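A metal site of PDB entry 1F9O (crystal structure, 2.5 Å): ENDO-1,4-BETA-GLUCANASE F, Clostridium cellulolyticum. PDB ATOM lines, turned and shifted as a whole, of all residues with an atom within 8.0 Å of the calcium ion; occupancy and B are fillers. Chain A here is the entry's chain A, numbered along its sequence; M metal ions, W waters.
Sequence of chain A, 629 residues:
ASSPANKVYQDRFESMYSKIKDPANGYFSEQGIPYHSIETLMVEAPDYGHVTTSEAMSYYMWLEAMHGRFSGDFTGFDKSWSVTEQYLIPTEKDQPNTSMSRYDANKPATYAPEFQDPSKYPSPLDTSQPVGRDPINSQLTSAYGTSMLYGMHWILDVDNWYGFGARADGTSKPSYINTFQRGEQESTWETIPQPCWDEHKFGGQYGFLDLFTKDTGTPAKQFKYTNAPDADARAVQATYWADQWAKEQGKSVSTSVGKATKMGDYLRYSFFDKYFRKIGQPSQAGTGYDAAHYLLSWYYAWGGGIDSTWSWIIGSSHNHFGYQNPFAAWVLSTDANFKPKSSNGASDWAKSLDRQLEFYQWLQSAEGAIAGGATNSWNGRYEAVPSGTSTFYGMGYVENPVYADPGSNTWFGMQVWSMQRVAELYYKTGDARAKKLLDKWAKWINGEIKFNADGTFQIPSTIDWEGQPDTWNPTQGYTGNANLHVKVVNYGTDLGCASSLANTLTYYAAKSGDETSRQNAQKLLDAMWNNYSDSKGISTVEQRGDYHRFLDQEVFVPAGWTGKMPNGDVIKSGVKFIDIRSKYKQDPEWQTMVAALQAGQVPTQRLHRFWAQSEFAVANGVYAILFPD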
ATOM      1  N   GLN A 116      16.859   8.921  24.983  1.00  0.00           N
ATOM      2  CA  GLN A 116      18.137   9.224  24.349  1.00  0.00           C
ATOM      3  C   GLN A 116      18.230  10.593  23.683  1.00  0.00           C
ATOM      4  O   GLN A 116      19.232  10.903  23.037  1.00  0.00           O
ATOM      5  CB  GLN A 116      18.469   8.126  23.339  1.00  0.00           C
ATOM      6  CG  GLN A 116      18.869   6.819  23.984  1.00  0.00           C
ATOM      7  CD  GLN A 116      17.831   6.281  24.922  1.00  0.00           C
ATOM      8  OE1 GLN A 116      16.729   5.937  24.498  1.00  0.00           O
ATOM      9  NE2 GLN A 116      18.153   6.212  26.207  1.00  0.00           N
ATOM     10  N   ASP A 117      17.184  11.400  23.826  1.00  0.00           N
ATOM     11  CA  ASP A 117      17.177  12.741  23.245  1.00  0.00           C
ATOM     12  C   ASP A 117      16.366  13.692  24.116  1.00  0.00           C
ATOM     13  O   ASP A 117      15.227  13.402  24.495  1.00  0.00           O
ATOM     14  CB  ASP A 117      16.581  12.739  21.833  1.00  0.00           C
ATOM     15  CG  ASP A 117      16.742  14.089  21.125  1.00  0.00           C
ATOM     16  OD1 ASP A 117      17.841  14.360  20.592  1.00  0.00           O
ATOM     17  OD2 ASP A 117      15.788  14.885  21.113  1.00  0.00           O
ATOM     18  N   PRO A 118      16.940  14.857  24.424  1.00  0.00           N
ATOM     19  CA  PRO A 118      16.324  15.893  25.251  1.00  0.00           C
ATOM     20  C   PRO A 118      14.917  16.324  24.823  1.00  0.00           C
ATOM     21  O   PRO A 118      14.136  16.808  25.650  1.00  0.00           O
ATOM     22  CB  PRO A 118      17.322  17.040  25.169  1.00  0.00           C
ATOM     23  CG  PRO A 118      18.628  16.332  25.028  1.00  0.00           C
ATOM     24  CD  PRO A 118      18.309  15.259  24.028  1.00  0.00           C
ATOM     25  N   GLY A 183      18.721  12.948  30.149  1.00  0.00           N
ATOM     26  CA  GLY A 183      19.377  11.912  29.355  1.00  0.00           C
ATOM     27  C   GLY A 183      20.809  12.034  28.875  1.00  0.00           C
ATOM     28  O   GLY A 183      21.485  13.037  29.067  1.00  0.00           O
ATOM     29  N   GLU A 184      21.241  10.956  28.209  1.00  0.00           N
ATOM     30  CA  GLU A 184      22.590  10.811  27.685  1.00  0.00           C
ATOM     31  C   GLU A 184      23.013  11.850  26.653  1.00  0.00           C
ATOM     32  O   GLU A 184      24.202  12.095  26.460  1.00  0.00           O
ATOM     33  CB  GLU A 184      22.773   9.420  27.099  1.00  0.00           C
ATOM     34  CG  GLU A 184      21.970   9.147  25.827  1.00  0.00           C
ATOM     35  CD  GLU A 184      22.185   7.753  25.268  1.00  0.00           C
ATOM     36  OE1 GLU A 184      21.638   6.780  25.836  1.00  0.00           O
ATOM     37  OE2 GLU A 184      22.917   7.618  24.264  1.00  0.00           O
ATOM     38  N   GLN A 185      22.044  12.446  25.982  1.00  0.00           N
ATOM     39  CA  GLN A 185      22.362  13.456  24.974  1.00  0.00           C
ATOM     40  C   GLN A 185      22.314  14.880  25.497  1.00  0.00           C
ATOM     41  O   GLN A 185      22.447  15.821  24.727  1.00  0.00           O
ATOM     42  CB  GLN A 185      21.427  13.321  23.768  1.00  0.00           C
ATOM     43  CG  GLN A 185      21.999  12.468  22.639  1.00  0.00           C
ATOM     44  CD  GLN A 185      23.390  12.938  22.201  1.00  0.00           C
ATOM     45  OE1 GLN A 185      23.666  14.139  22.122  1.00  0.00           O
ATOM     46  NE2 GLN A 185      24.266  11.989  21.887  1.00  0.00           N
ATOM     47  N   GLU A 186      22.125  15.055  26.804  1.00  0.00           N
ATOM     48  CA  GLU A 186      22.077  16.405  27.359  1.00  0.00           C
ATOM     49  C   GLU A 186      23.427  16.801  27.981  1.00  0.00           C
ATOM     50  O   GLU A 186      23.756  16.395  29.099  1.00  0.00           O
ATOM     51  CB  GLU A 186      20.957  16.529  28.397  1.00  0.00           C
ATOM     52  CG  GLU A 186      20.830  17.919  28.966  1.00  0.00           C
ATOM     53  CD  GLU A 186      19.834  17.992  30.103  1.00  0.00           C
ATOM     54  OE1 GLU A 186      19.936  17.148  31.020  1.00  0.00           O
ATOM     55  OE2 GLU A 186      18.978  18.904  30.102  1.00  0.00           O
ATOM     56  N   SER A 187      24.197  17.585  27.244  1.00  0.00           N
ATOM     57  CA  SER A 187      25.511  18.062  27.662  1.00  0.00           C
ATOM     58  C   SER A 187      25.412  19.251  28.595  1.00  0.00           C
ATOM     59  O   SER A 187      24.321  19.730  28.888  1.00  0.00           O
ATOM     60  CB  SER A 187      26.304  18.462  26.431  1.00  0.00           C
ATOM     61  OG  SER A 187      25.674  19.570  25.809  1.00  0.00           O
ATOM     62  N   THR A 188      26.566  19.745  29.052  1.00  0.00           N
ATOM     63  CA  THR A 188      26.612  20.912  29.933  1.00  0.00           C
ATOM     64  C   THR A 188      25.899  22.045  29.220  1.00  0.00           C
ATOM     65  O   THR A 188      25.279  22.904  29.852  1.00  0.00           O
ATOM     66  CB  THR A 188      28.057  21.408  30.201  1.00  0.00           C
ATOM     67  OG1 THR A 188      29.005  20.525  29.590  1.00  0.00           O
ATOM     68  CG2 THR A 188      28.330  21.491  31.675  1.00  0.00           C
ATOM     69  N   TRP A 189      25.992  22.025  27.896  1.00  0.00           N
ATOM     70  CA  TRP A 189      25.416  23.040  27.037  1.00  0.00           C
ATOM     71  C   TRP A 189      23.907  22.980  26.769  1.00  0.00           C
ATOM     72  O   TRP A 189      23.333  23.987  26.369  1.00  0.00           O
ATOM     73  CB  TRP A 189      26.122  23.029  25.686  1.00  0.00           C
ATOM     74  CG  TRP A 189      27.605  23.115  25.762  1.00  0.00           C
ATOM     75  CD1 TRP A 189      28.480  22.078  25.714  1.00  0.00           C
ATOM     76  CD2 TRP A 189      28.371  24.304  25.926  1.00  0.00           C
ATOM     77  NE1 TRP A 189      29.769  22.548  25.823  1.00  0.00           N
ATOM     78  CE2 TRP A 189      29.730  23.909  25.957  1.00  0.00           C
ATOM     79  CE3 TRP A 189      28.047  25.659  26.031  1.00  0.00           C
ATOM     80  CZ2 TRP A 189      30.765  24.835  26.107  1.00  0.00           C
ATOM     81  CZ3 TRP A 189      29.075  26.582  26.175  1.00  0.00           C
ATOM     82  CH2 TRP A 189      30.431  26.157  26.206  1.00  0.00           C
ATOM     83  N   GLU A 190      23.288  21.834  26.979  1.00  0.00           N
ATOM     84  CA  GLU A 190      21.854  21.682  26.661  1.00  0.00           C
ATOM     85  C   GLU A 190      20.884  21.652  27.845  1.00  0.00           C
ATOM     86  O   GLU A 190      19.710  21.293  27.678  1.00  0.00           O
ATOM     87  CB  GLU A 190      21.674  20.432  25.783  1.00  0.00           C
ATOM     88  CG  GLU A 190      22.421  20.504  24.442  1.00  0.00           C
ATOM     89  CD  GLU A 190      22.687  19.153  23.802  1.00  0.00           C
ATOM     90  OE1 GLU A 190      21.793  18.628  23.094  1.00  0.00           O
ATOM     91  OE2 GLU A 190      23.781  18.602  24.010  1.00  0.00           O
ATOM     92  N   ALA A 404      26.806  10.692  26.375  1.00  0.00           N
ATOM     93  CA  ALA A 404      27.323  10.423  25.038  1.00  0.00           C
ATOM     94  C   ALA A 404      27.812  11.685  24.365  1.00  0.00           C
ATOM     95  O   ALA A 404      28.394  11.623  23.283  1.00  0.00           O
ATOM     96  CB  ALA A 404      26.217   9.786  24.195  1.00  0.00           C
ATOM     97  N   ASP A 405      27.591  12.829  24.992  1.00  0.00           N
ATOM     98  CA  ASP A 405      27.973  14.117  24.420  1.00  0.00           C
ATOM     99  C   ASP A 405      28.758  15.011  25.391  1.00  0.00           C
ATOM    100  O   ASP A 405      28.207  15.938  25.975  1.00  0.00           O
ATOM    101  CB  ASP A 405      26.689  14.815  23.938  1.00  0.00           C
ATOM    102  CG  ASP A 405      26.943  16.174  23.327  1.00  0.00           C
ATOM    103  OD1 ASP A 405      28.103  16.496  22.973  1.00  0.00           O
ATOM    104  OD2 ASP A 405      25.952  16.927  23.183  1.00  0.00           O
ATOM    105  N   PRO A 406      30.055  14.734  25.576  1.00  0.00           N
ATOM    106  CA  PRO A 406      30.829  13.661  24.950  1.00  0.00           C
ATOM    107  C   PRO A 406      30.777  12.401  25.811  1.00  0.00           C
ATOM    108  O   PRO A 406      30.371  12.458  26.960  1.00  0.00           O
ATOM    109  CB  PRO A 406      32.222  14.256  24.879  1.00  0.00           C
ATOM    110  CG  PRO A 406      32.307  14.944  26.216  1.00  0.00           C
ATOM    111  CD  PRO A 406      30.963  15.658  26.287  1.00  0.00           C
ATOM    112  N   ARG A 549      29.582  26.467  21.200  1.00  0.00           N
ATOM    113  CA  ARG A 549      28.258  26.061  21.642  1.00  0.00           C
ATOM    114  C   ARG A 549      27.682  27.164  22.537  1.00  0.00           C
ATOM    115  O   ARG A 549      26.489  27.203  22.820  1.00  0.00           O
ATOM    116  CB  ARG A 549      28.346  24.723  22.368  1.00  0.00           C
ATOM    117  CG  ARG A 549      29.032  23.679  21.478  1.00  0.00           C
ATOM    118  CD  ARG A 549      29.022  22.293  22.067  1.00  0.00           C
ATOM    119  NE  ARG A 549      27.688  21.702  22.114  1.00  0.00           N
ATOM    120  CZ  ARG A 549      27.458  20.413  22.323  1.00  0.00           C
ATOM    121  NH1 ARG A 549      28.489  19.583  22.486  1.00  0.00           N
ATOM    122  NH2 ARG A 549      26.227  19.954  22.383  1.00  0.00           N
ATOM    123  N   GLN A 553      24.626  26.609  20.267  1.00  0.00           N
ATOM    124  CA  GLN A 553      23.858  25.504  20.850  1.00  0.00           C
ATOM    125  C   GLN A 553      22.429  25.864  21.245  1.00  0.00           C
ATOM    126  O   GLN A 553      22.184  26.714  22.095  1.00  0.00           O
ATOM    127  CB  GLN A 553      24.560  24.939  22.074  1.00  0.00           C
ATOM    128  CG  GLN A 553      23.804  23.779  22.699  1.00  0.00           C
ATOM    129  CD  GLN A 553      23.758  22.556  21.795  1.00  0.00           C
ATOM    130  OE1 GLN A 553      24.790  21.951  21.515  1.00  0.00           O
ATOM    131  NE2 GLN A 553      22.572  22.209  21.328  1.00  0.00           N
ATOM    132  N   GLU A 554      21.493  25.165  20.615  1.00  0.00           N
ATOM    133  CA  GLU A 554      20.076  25.357  20.873  1.00  0.00           C
ATOM    134  C   GLU A 554      19.688  24.546  22.106  1.00  0.00           C
ATOM    135  O   GLU A 554      20.162  23.422  22.288  1.00  0.00           O
ATOM    136  CB  GLU A 554      19.263  24.881  19.654  1.00  0.00           C
ATOM    137  CG  GLU A 554      17.935  25.579  19.470  1.00  0.00           C
ATOM    138  CD  GLU A 554      17.148  25.044  18.295  1.00  0.00           C
ATOM    139  OE1 GLU A 554      17.664  25.098  17.159  1.00  0.00           O
ATOM    140  OE2 GLU A 554      16.013  24.550  18.515  1.00  0.00           O
HETATM  141 CA    CA M   1      23.453  16.641  22.598  1.00  0.00          CA
HETATM  142  O   HOH W   1      23.907  17.837  20.596  1.00  0.00           O
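OE2 of Glu 190 sits close to NH2 of Arg 549. NH1 of Arg 549 lies within salt-bridge range of OD1 of Asp 405, at 3.1 Å. N of Glu 190 is in hydrogen-bond range of OG of Ser 187 (3.5 Å).
Of the 17 residues printed, 3 come within 4 Å of the calcium ion. The nearest printed residue that does not touch the calcium ion is Arg 549 (4.3 Å).
The calcium ion is bound by water W1 (2.4 Å), the side-chain carboxylate (OE2) of Glu 190 (2.4 Å), the backbone carbonyl oxygen (O) of Gln 185 (2.5 Å), the side-chain amide oxygen (OE1) of Gln 185 (2.6 Å), the side-chain carboxylate (OD2) of Asp 405 (2.6 Å) and the side-chain carboxylate (OE1) of Glu 190 (2.6 Å).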
